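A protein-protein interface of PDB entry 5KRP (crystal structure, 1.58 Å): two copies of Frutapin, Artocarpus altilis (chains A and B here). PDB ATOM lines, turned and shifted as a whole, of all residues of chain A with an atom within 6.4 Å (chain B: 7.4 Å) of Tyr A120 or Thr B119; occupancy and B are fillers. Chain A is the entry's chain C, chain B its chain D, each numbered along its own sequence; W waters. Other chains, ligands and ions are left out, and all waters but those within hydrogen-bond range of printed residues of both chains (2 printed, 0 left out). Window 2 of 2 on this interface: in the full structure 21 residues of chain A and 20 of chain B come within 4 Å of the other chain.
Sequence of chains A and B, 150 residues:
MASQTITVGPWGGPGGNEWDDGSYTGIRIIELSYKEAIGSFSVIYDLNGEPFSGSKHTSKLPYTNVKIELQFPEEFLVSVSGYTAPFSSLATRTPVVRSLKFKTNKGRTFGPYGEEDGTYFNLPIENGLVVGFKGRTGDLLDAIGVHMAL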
ATOM      1  N   TRP A  11      -4.761  22.209 -12.203  1.00  0.00           N
ATOM      2  CA  TRP A  11      -5.580  23.320 -11.710  1.00  0.00           C
ATOM      3  C   TRP A  11      -5.220  24.588 -12.462  1.00  0.00           C
ATOM      4  O   TRP A  11      -4.030  24.965 -12.565  1.00  0.00           O
ATOM      5  CB  TRP A  11      -5.270  23.505 -10.280  1.00  0.00           C
ATOM      6  CG  TRP A  11      -5.669  22.341  -9.394  1.00  0.00           C
ATOM      7  CD1 TRP A  11      -6.931  22.112  -8.832  1.00  0.00           C
ATOM      8  CD2 TRP A  11      -4.834  21.239  -8.974  1.00  0.00           C
ATOM      9  NE1 TRP A  11      -6.917  20.919  -8.144  1.00  0.00           N
ATOM     10  CE2 TRP A  11      -5.654  20.386  -8.146  1.00  0.00           C
ATOM     11  CE3 TRP A  11      -3.516  20.869  -9.233  1.00  0.00           C
ATOM     12  CZ2 TRP A  11      -5.169  19.228  -7.547  1.00  0.00           C
ATOM     13  CZ3 TRP A  11      -3.007  19.729  -8.584  1.00  0.00           C
ATOM     14  CH2 TRP A  11      -3.878  18.872  -7.818  1.00  0.00           C
ATOM     15  N   SER A  79       2.491  19.600   0.732  1.00  0.00           N
ATOM     16  CA  SER A  79       1.310  20.348   0.329  1.00  0.00           C
ATOM     17  C   SER A  79       1.680  21.251  -0.852  1.00  0.00           C
ATOM     18  O   SER A  79       2.710  21.909  -0.814  1.00  0.00           O
ATOM     19  CB  SER A  79       0.735  21.231   1.472  1.00  0.00           C
ATOM     20  OG  SER A  79      -0.361  22.018   1.035  1.00  0.00           O
ATOM     21  N   SER A  81      -0.641  24.190  -2.852  1.00  0.00           N
ATOM     22  CA  SER A  81      -1.965  24.867  -2.868  1.00  0.00           C
ATOM     23  C   SER A  81      -1.868  26.205  -3.617  1.00  0.00           C
ATOM     24  O   SER A  81      -0.761  26.633  -4.054  1.00  0.00           O
ATOM     25  CB  SER A  81      -2.523  25.034  -1.462  1.00  0.00           C
ATOM     26  OG  SER A  81      -1.749  25.925  -0.698  1.00  0.00           O
ATOM     27  N   GLY A  82      -2.991  26.815  -3.810  1.00  0.00           N
ATOM     28  CA  GLY A  82      -3.037  28.085  -4.552  1.00  0.00           C
ATOM     29  C   GLY A  82      -4.385  28.538  -4.930  1.00  0.00           C
ATOM     30  O   GLY A  82      -5.404  27.995  -4.458  1.00  0.00           O
ATOM     31  N   TYR A  83      -4.417  29.521  -5.841  1.00  0.00           N
ATOM     32  CA  TYR A  83      -5.691  30.056  -6.320  1.00  0.00           C
ATOM     33  C   TYR A  83      -5.640  30.186  -7.796  1.00  0.00           C
ATOM     34  O   TYR A  83      -4.620  30.601  -8.359  1.00  0.00           O
ATOM     35  CB  TYR A  83      -5.984  31.470  -5.725  1.00  0.00           C
ATOM     36  CG  TYR A  83      -6.391  31.430  -4.298  1.00  0.00           C
ATOM     37  CD1 TYR A  83      -5.428  31.218  -3.308  1.00  0.00           C
ATOM     38  CD2 TYR A  83      -7.721  31.667  -3.917  1.00  0.00           C
ATOM     39  CE1 TYR A  83      -5.796  31.114  -1.960  1.00  0.00           C
ATOM     40  CE2 TYR A  83      -8.086  31.605  -2.572  1.00  0.00           C
ATOM     41  CZ  TYR A  83      -7.138  31.376  -1.622  1.00  0.00           C
ATOM     42  OH  TYR A  83      -7.616  31.322  -0.329  1.00  0.00           O
ATOM     43  N   THR A  84      -6.764  29.931  -8.434  1.00  0.00           N
ATOM     44  CA  THR A  84      -6.957  30.175  -9.863  1.00  0.00           C
ATOM     45  C   THR A  84      -8.133  31.076 -10.131  1.00  0.00           C
ATOM     46  O   THR A  84      -9.157  30.985  -9.420  1.00  0.00           O
ATOM     47  CB  THR A  84      -7.117  28.872 -10.700  1.00  0.00           C
ATOM     48  OG1 THR A  84      -8.307  28.172 -10.295  1.00  0.00           O
ATOM     49  CG2 THR A  84      -5.863  27.993 -10.512  1.00  0.00           C
ATOM     50  N   LYS A 101       1.442  28.237  -3.093  1.00  0.00           N
ATOM     51  CA  LYS A 101       2.011  28.096  -1.765  1.00  0.00           C
ATOM     52  C   LYS A 101       2.430  26.655  -1.583  1.00  0.00           C
ATOM     53  O   LYS A 101       1.712  25.747  -2.066  1.00  0.00           O
ATOM     54  CB  LYS A 101       0.980  28.526  -0.684  1.00  0.00           C
ATOM     55  CG  LYS A 101       1.550  28.452   0.721  1.00  0.00           C
ATOM     56  CD  LYS A 101       0.681  29.198   1.728  1.00  0.00           C
ATOM     57  CE  LYS A 101      -0.502  28.386   2.116  1.00  0.00           C
ATOM     58  NZ  LYS A 101      -1.148  29.093   3.281  1.00  0.00           N
ATOM     59  N   GLU A 116      -4.085  35.961  -3.692  1.00  0.00           N
ATOM     60  CA  GLU A 116      -5.119  34.970  -3.351  1.00  0.00           C
ATOM     61  C   GLU A 116      -6.536  35.361  -3.743  1.00  0.00           C
ATOM     62  O   GLU A 116      -7.396  35.622  -2.909  1.00  0.00           O
ATOM     63  CB  GLU A 116      -4.983  34.598  -1.892  1.00  0.00           C
ATOM     64  CG  GLU A 116      -3.624  33.975  -1.598  1.00  0.00           C
ATOM     65  CD  GLU A 116      -3.555  33.381  -0.213  1.00  0.00           C
ATOM     66  OE1 GLU A 116      -4.120  34.000   0.689  1.00  0.00           O
ATOM     67  OE2 GLU A 116      -2.926  32.323  -0.003  1.00  0.00           O
ATOM     68  N   ASP A 117      -6.770  35.355  -5.033  1.00  0.00           N
ATOM     69  CA  ASP A 117      -8.028  35.743  -5.602  1.00  0.00           C
ATOM     70  C   ASP A 117      -8.567  34.571  -6.376  1.00  0.00           C
ATOM     71  O   ASP A 117      -7.825  33.954  -7.171  1.00  0.00           O
ATOM     72  CB  ASP A 117      -7.796  36.965  -6.544  1.00  0.00           C
ATOM     73  CG  ASP A 117      -9.093  37.728  -6.886  1.00  0.00           C
ATOM     74  OD1 ASP A 117      -9.996  37.783  -6.040  1.00  0.00           O
ATOM     75  OD2 ASP A 117      -9.210  38.271  -8.008  1.00  0.00           O
ATOM     76  N   GLY A 118      -9.864  34.287  -6.167  1.00  0.00           N
ATOM     77  CA  GLY A 118     -10.607  33.322  -6.975  1.00  0.00           C
ATOM     78  C   GLY A 118     -10.805  32.006  -6.233  1.00  0.00           C
ATOM     79  O   GLY A 118     -11.225  32.021  -5.084  1.00  0.00           O
ATOM     80  N   THR A 119     -10.589  30.888  -6.930  1.00  0.00           N
ATOM     81  CA  THR A 119     -10.889  29.537  -6.445  1.00  0.00           C
ATOM     82  C   THR A 119      -9.639  28.872  -5.868  1.00  0.00           C
ATOM     83  O   THR A 119      -8.616  28.663  -6.588  1.00  0.00           O
ATOM     84  CB  THR A 119     -11.464  28.728  -7.597  1.00  0.00           C
ATOM     85  OG1 THR A 119     -12.610  29.428  -8.131  1.00  0.00           O
ATOM     86  CG2 THR A 119     -11.902  27.314  -7.134  1.00  0.00           C
ATOM     87  N   TYR A 120      -9.687  28.643  -4.553  1.00  0.00           N
ATOM     88  CA  TYR A 120      -8.636  27.890  -3.856  1.00  0.00           C
ATOM     89  C   TYR A 120      -8.554  26.450  -4.371  1.00  0.00           C
ATOM     90  O   TYR A 120      -9.591  25.848  -4.690  1.00  0.00           O
ATOM     91  CB  TYR A 120      -8.945  27.892  -2.375  1.00  0.00           C
ATOM     92  CG  TYR A 120      -8.013  27.160  -1.449  1.00  0.00           C
ATOM     93  CD1 TYR A 120      -6.731  27.608  -1.208  1.00  0.00           C
ATOM     94  CD2 TYR A 120      -8.478  26.041  -0.697  1.00  0.00           C
ATOM     95  CE1 TYR A 120      -5.921  27.023  -0.286  1.00  0.00           C
ATOM     96  CE2 TYR A 120      -7.663  25.471   0.236  1.00  0.00           C
ATOM     97  CZ  TYR A 120      -6.382  25.946   0.424  1.00  0.00           C
ATOM     98  OH  TYR A 120      -5.555  25.356   1.307  1.00  0.00           O
ATOM     99  N   PHE A 121      -7.314  25.916  -4.483  1.00  0.00           N
ATOM    100  CA  PHE A 121      -7.049  24.482  -4.663  1.00  0.00           C
ATOM    101  C   PHE A 121      -6.020  24.066  -3.687  1.00  0.00           C
ATOM    102  O   PHE A 121      -5.192  24.871  -3.238  1.00  0.00           O
ATOM    103  CB  PHE A 121      -6.657  24.094  -6.073  1.00  0.00           C
ATOM    104  CG  PHE A 121      -5.261  24.583  -6.526  1.00  0.00           C
ATOM    105  CD1 PHE A 121      -5.051  25.873  -7.065  1.00  0.00           C
ATOM    106  CD2 PHE A 121      -4.145  23.747  -6.361  1.00  0.00           C
ATOM    107  CE1 PHE A 121      -3.758  26.270  -7.501  1.00  0.00           C
ATOM    108  CE2 PHE A 121      -2.898  24.146  -6.806  1.00  0.00           C
ATOM    109  CZ  PHE A 121      -2.694  25.410  -7.327  1.00  0.00           C
ATOM    110  N   ASN A 122      -6.050  22.782  -3.331  1.00  0.00           N
ATOM    111  CA  ASN A 122      -5.207  22.334  -2.252  1.00  0.00           C
ATOM    112  C   ASN A 122      -4.974  20.839  -2.419  1.00  0.00           C
ATOM    113  O   ASN A 122      -5.962  20.056  -2.497  1.00  0.00           O
ATOM    114  CB  ASN A 122      -6.011  22.542  -1.004  1.00  0.00           C
ATOM    115  CG  ASN A 122      -5.365  22.007   0.195  1.00  0.00           C
ATOM    116  OD1 ASN A 122      -4.149  21.988   0.287  1.00  0.00           O
ATOM    117  ND2 ASN A 122      -6.189  21.563   1.154  1.00  0.00           N
ATOM    118  N   TRP B  11      -9.389  16.140   2.973  1.00  0.00           N
ATOM    119  CA  TRP B  11     -10.087  17.434   2.875  1.00  0.00           C
ATOM    120  C   TRP B  11     -11.183  17.418   3.939  1.00  0.00           C
ATOM    121  O   TRP B  11     -12.004  16.459   3.964  1.00  0.00           O
ATOM    122  CB  TRP B  11     -10.613  17.590   1.504  1.00  0.00           C
ATOM    123  CG  TRP B  11      -9.515  17.779   0.472  1.00  0.00           C
ATOM    124  CD1 TRP B  11      -8.849  18.956   0.164  1.00  0.00           C
ATOM    125  CD2 TRP B  11      -8.951  16.774  -0.400  1.00  0.00           C
ATOM    126  NE1 TRP B  11      -7.919  18.733  -0.890  1.00  0.00           N
ATOM    127  CE2 TRP B  11      -7.977  17.411  -1.239  1.00  0.00           C
ATOM    128  CE3 TRP B  11      -9.202  15.397  -0.580  1.00  0.00           C
ATOM    129  CZ2 TRP B  11      -7.235  16.706  -2.198  1.00  0.00           C
ATOM    130  CZ3 TRP B  11      -8.466  14.700  -1.538  1.00  0.00           C
ATOM    131  CH2 TRP B  11      -7.470  15.366  -2.314  1.00  0.00           C
ATOM    132  N   GLY B  82     -15.710  18.562  -3.872  1.00  0.00           N
ATOM    133  CA  GLY B  82     -16.744  18.839  -2.883  1.00  0.00           C
ATOM    134  C   GLY B  82     -16.468  20.106  -2.172  1.00  0.00           C
ATOM    135  O   GLY B  82     -15.645  20.929  -2.659  1.00  0.00           O
ATOM    136  N   TYR B  83     -17.168  20.274  -1.040  1.00  0.00           N
ATOM    137  CA  TYR B  83     -17.034  21.445  -0.199  1.00  0.00           C
ATOM    138  C   TYR B  83     -16.896  21.070   1.230  1.00  0.00           C
ATOM    139  O   TYR B  83     -17.593  20.135   1.704  1.00  0.00           O
ATOM    140  CB  TYR B  83     -18.272  22.353  -0.306  1.00  0.00           C
ATOM    141  CG  TYR B  83     -18.338  23.100  -1.593  1.00  0.00           C
ATOM    142  CD1 TYR B  83     -18.649  22.463  -2.754  1.00  0.00           C
ATOM    143  CD2 TYR B  83     -18.009  24.465  -1.649  1.00  0.00           C
ATOM    144  CE1 TYR B  83     -18.691  23.147  -3.951  1.00  0.00           C
ATOM    145  CE2 TYR B  83     -18.033  25.159  -2.862  1.00  0.00           C
ATOM    146  CZ  TYR B  83     -18.365  24.502  -3.995  1.00  0.00           C
ATOM    147  OH  TYR B  83     -18.386  25.213  -5.202  1.00  0.00           O
ATOM    148  N   THR B  84     -16.062  21.813   1.949  1.00  0.00           N
ATOM    149  CA  THR B  84     -15.873  21.604   3.383  1.00  0.00           C
ATOM    150  C   THR B  84     -16.118  22.964   4.131  1.00  0.00           C
ATOM    151  O   THR B  84     -15.780  24.030   3.608  1.00  0.00           O
ATOM    152  CB  THR B  84     -14.516  21.014   3.757  1.00  0.00           C
ATOM    153  OG1 THR B  84     -13.458  21.949   3.475  1.00  0.00           O
ATOM    154  CG2 THR B  84     -14.264  19.731   2.991  1.00  0.00           C
ATOM    155  N   ALA B  85     -16.727  22.902   5.321  1.00  0.00           N
ATOM    156  CA  ALA B  85     -17.102  24.110   6.092  1.00  0.00           C
ATOM    157  C   ALA B  85     -17.552  23.730   7.481  1.00  0.00           C
ATOM    158  O   ALA B  85     -17.990  22.597   7.703  1.00  0.00           O
ATOM    159  CB  ALA B  85     -18.221  24.830   5.403  1.00  0.00           C
ATOM    160  N   PRO B  86     -17.458  24.665   8.429  1.00  0.00           N
ATOM    161  CA  PRO B  86     -18.231  24.451   9.669  1.00  0.00           C
ATOM    162  C   PRO B  86     -19.724  24.222   9.358  1.00  0.00           C
ATOM    163  O   PRO B  86     -20.261  24.554   8.281  1.00  0.00           O
ATOM    164  CB  PRO B  86     -17.975  25.756  10.467  1.00  0.00           C
ATOM    165  CG  PRO B  86     -16.799  26.376   9.862  1.00  0.00           C
ATOM    166  CD  PRO B  86     -16.860  26.019   8.390  1.00  0.00           C
ATOM    167  N   VAL B  96     -16.419  20.254   8.351  1.00  0.00           N
ATOM    168  CA  VAL B  96     -16.865  18.906   7.975  1.00  0.00           C
ATOM    169  C   VAL B  96     -17.151  18.898   6.511  1.00  0.00           C
ATOM    170  O   VAL B  96     -17.145  19.932   5.873  1.00  0.00           O
ATOM    171  CB  VAL B  96     -18.114  18.430   8.782  1.00  0.00           C
ATOM    172  CG1 VAL B  96     -17.858  18.553  10.246  1.00  0.00           C
ATOM    173  CG2 VAL B  96     -19.334  19.177   8.380  1.00  0.00           C
ATOM    174  N   ARG B  98     -19.366  19.057   3.548  1.00  0.00           N
ATOM    175  CA  ARG B  98     -20.669  19.581   3.304  1.00  0.00           C
ATOM    176  C   ARG B  98     -21.220  19.019   2.008  1.00  0.00           C
ATOM    177  O   ARG B  98     -22.438  18.823   1.870  1.00  0.00           O
ATOM    178  CB  ARG B  98     -20.689  21.147   3.304  1.00  0.00           C
ATOM    179  CG  ARG B  98     -20.225  21.835   4.571  1.00  0.00           C
ATOM    180  CD  ARG B  98     -21.056  21.450   5.838  1.00  0.00           C
ATOM    181  NE  ARG B  98     -22.427  21.824   5.554  1.00  0.00           N
ATOM    182  CZ  ARG B  98     -22.949  23.044   5.693  1.00  0.00           C
ATOM    183  NH1 ARG B  98     -22.236  24.061   6.212  1.00  0.00           N
ATOM    184  NH2 ARG B  98     -24.175  23.243   5.263  1.00  0.00           N
ATOM    185  N   SER B  99     -20.369  18.725   1.016  1.00  0.00           N
ATOM    186  CA  SER B  99     -20.847  18.245  -0.243  1.00  0.00           C
ATOM    187  C   SER B  99     -19.788  17.367  -0.944  1.00  0.00           C
ATOM    188  O   SER B  99     -18.604  17.630  -0.739  1.00  0.00           O
ATOM    189  CB  SER B  99     -21.114  19.434  -1.161  1.00  0.00           C
ATOM    190  OG  SER B  99     -21.677  19.006  -2.365  1.00  0.00           O
ATOM    191  N   GLU B 116     -23.373  22.892  -1.235  1.00  0.00           N
ATOM    192  CA  GLU B 116     -22.119  23.531  -1.680  1.00  0.00           C
ATOM    193  C   GLU B 116     -21.838  24.821  -0.934  1.00  0.00           C
ATOM    194  O   GLU B 116     -21.866  25.902  -1.515  1.00  0.00           O
ATOM    195  CB  GLU B 116     -22.129  23.717  -3.215  1.00  0.00           C
ATOM    196  CG  GLU B 116     -22.288  22.384  -3.883  1.00  0.00           C
ATOM    197  CD  GLU B 116     -22.058  22.403  -5.350  1.00  0.00           C
ATOM    198  OE1 GLU B 116     -22.631  23.306  -5.971  1.00  0.00           O
ATOM    199  OE2 GLU B 116     -21.277  21.573  -5.873  1.00  0.00           O
ATOM    200  N   ASP B 117     -21.482  24.701   0.325  1.00  0.00           N
ATOM    201  CA  ASP B 117     -21.195  25.848   1.194  1.00  0.00           C
ATOM    202  C   ASP B 117     -19.798  25.709   1.688  1.00  0.00           C
ATOM    203  O   ASP B 117     -19.439  24.626   2.181  1.00  0.00           O
ATOM    204  CB  ASP B 117     -22.132  25.857   2.421  1.00  0.00           C
ATOM    205  CG  ASP B 117     -22.149  27.241   3.165  1.00  0.00           C
ATOM    206  OD1 ASP B 117     -21.722  28.286   2.602  1.00  0.00           O
ATOM    207  OD2 ASP B 117     -22.628  27.272   4.325  1.00  0.00           O
ATOM    208  N   GLY B 118     -18.997  26.776   1.573  1.00  0.00           N
ATOM    209  CA  GLY B 118     -17.709  26.866   2.195  1.00  0.00           C
ATOM    210  C   GLY B 118     -16.580  26.796   1.171  1.00  0.00           C
ATOM    211  O   GLY B 118     -16.667  27.425   0.125  1.00  0.00           O
ATOM    212  N   THR B 119     -15.563  26.000   1.483  1.00  0.00           N
ATOM    213  CA  THR B 119     -14.349  25.911   0.657  1.00  0.00           C
ATOM    214  C   THR B 119     -14.417  24.707  -0.317  1.00  0.00           C
ATOM    215  O   THR B 119     -14.512  23.574   0.136  1.00  0.00           O
ATOM    216  CB  THR B 119     -13.135  25.784   1.564  1.00  0.00           C
ATOM    217  OG1 THR B 119     -13.113  26.861   2.512  1.00  0.00           O
ATOM    218  CG2 THR B 119     -11.809  25.793   0.768  1.00  0.00           C
ATOM    219  N   TYR B 120     -14.420  24.984  -1.636  1.00  0.00           N
ATOM    220  CA  TYR B 120     -14.359  23.976  -2.651  1.00  0.00           C
ATOM    221  C   TYR B 120     -13.000  23.225  -2.565  1.00  0.00           C
ATOM    222  O   TYR B 120     -11.976  23.765  -2.094  1.00  0.00           O
ATOM    223  CB  TYR B 120     -14.604  24.608  -3.994  1.00  0.00           C
ATOM    224  CG  TYR B 120     -14.484  23.769  -5.242  1.00  0.00           C
ATOM    225  CD1 TYR B 120     -15.442  22.834  -5.594  1.00  0.00           C
ATOM    226  CD2 TYR B 120     -13.430  24.010  -6.167  1.00  0.00           C
ATOM    227  CE1 TYR B 120     -15.365  22.136  -6.763  1.00  0.00           C
ATOM    228  CE2 TYR B 120     -13.377  23.327  -7.319  1.00  0.00           C
ATOM    229  CZ  TYR B 120     -14.333  22.396  -7.623  1.00  0.00           C
ATOM    230  OH  TYR B 120     -14.300  21.685  -8.748  1.00  0.00           O
ATOM    231  N   PHE B 121     -13.040  21.906  -2.873  1.00  0.00           N
ATOM    232  CA  PHE B 121     -11.832  21.098  -3.105  1.00  0.00           C
ATOM    233  C   PHE B 121     -12.017  20.280  -4.351  1.00  0.00           C
ATOM    234  O   PHE B 121     -13.163  19.961  -4.767  1.00  0.00           O
ATOM    235  CB  PHE B 121     -11.384  20.211  -1.951  1.00  0.00           C
ATOM    236  CG  PHE B 121     -12.288  19.011  -1.682  1.00  0.00           C
ATOM    237  CD1 PHE B 121     -13.388  19.138  -0.847  1.00  0.00           C
ATOM    238  CD2 PHE B 121     -12.025  17.771  -2.258  1.00  0.00           C
ATOM    239  CE1 PHE B 121     -14.236  18.063  -0.601  1.00  0.00           C
ATOM    240  CE2 PHE B 121     -12.867  16.707  -2.036  1.00  0.00           C
ATOM    241  CZ  PHE B 121     -13.945  16.839  -1.169  1.00  0.00           C
ATOM    242  N   ASN B 122     -10.877  19.926  -4.995  1.00  0.00           N
ATOM    243  CA  ASN B 122     -11.045  19.275  -6.288  1.00  0.00           C
ATOM    244  C   ASN B 122      -9.772  18.500  -6.616  1.00  0.00           C
ATOM    245  O   ASN B 122      -8.662  19.096  -6.548  1.00  0.00           O
ATOM    246  CB  ASN B 122     -11.298  20.383  -7.259  1.00  0.00           C
ATOM    247  CG  ASN B 122     -11.217  19.965  -8.622  1.00  0.00           C
ATOM    248  OD1 ASN B 122     -11.734  18.902  -8.972  1.00  0.00           O
ATOM    249  ND2 ASN B 122     -10.562  20.800  -9.466  1.00  0.00           N
HETATM  250  O   HOH W   1      -8.271  21.108  -4.159  1.00  0.00           O
HETATM  251  O   HOH W   2     -11.723  26.382  -3.136  1.00  0.00           O
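The indole nitrogen (NE1) of Trp A11 is in hydrogen-bond range of the backbone carbonyl oxygen (O) of Asn B122 (3.0 Å). The indole nitrogen (NE1) of Trp B11 lies within hydrogen-bond range of the backbone carbonyl oxygen (O) of Asn A122 (2.9 Å).
The backbone NH (N) of Thr A119 sits at hydrogen-bond distance from the backbone carbonyl oxygen (O) of Thr A84, 2.9 Å away. O of Thr B84 is in hydrogen-bond range of N of Thr B119 (2.9 Å).
Among the printed residues, merely in contact across the chains: Thr A119 with Tyr B120 and Tyr A120 with Thr B119.
Of chain A, only Tyr A120 comes within 4 Å of Thr B119. Of the printed residues of chain B, Asn A122 touches Trp B11 (2.9 Å). Of the printed residues of chain B, Thr A119 touches Tyr B120 (3.8 Å). Printed residues of chain A within 4 Å of Tyr B120: Thr A119 (3.8 Å). Printed residues of chain A within 4 Å of Trp B11: Asn A122. Printed residues of chain A within 4 Å of Asn B122: Trp A11.
Hydrophobic or aromatic side chains of chain B within 4 Å of the printed part of chain A: Trp B11 and Tyr B120. Of the 14 printed residues of chain A, 4 touch a printed residue of chain B. Along chain A the printed residues that touch a printed residue of chain B span positions 11 to 122. Among the printed residues, 4 pairs touch across the chains.
Trp A11 touches Asn B122, and with the chains exchanged Asn A122 touches Trp B11. Thr A119 touches Tyr B120, and with the chains exchanged Tyr A120 touches Thr B119. Positions printed for both chains: 11, 82, 83, 84, 116, 117, 118, 119, 120, 121 and 122. Of the 4 pairs that touch across the chains among the printed residues, 4 have their exchanged pair printed and touching as well.
Water W2 bridges the backbone carbonyl oxygen (O) of Tyr A120 (2.7 Å) and the backbone carbonyl oxygen (O) of Tyr B120 (2.8 Å). Water W1 bridges N of Asn A122 and N of Asn B122.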
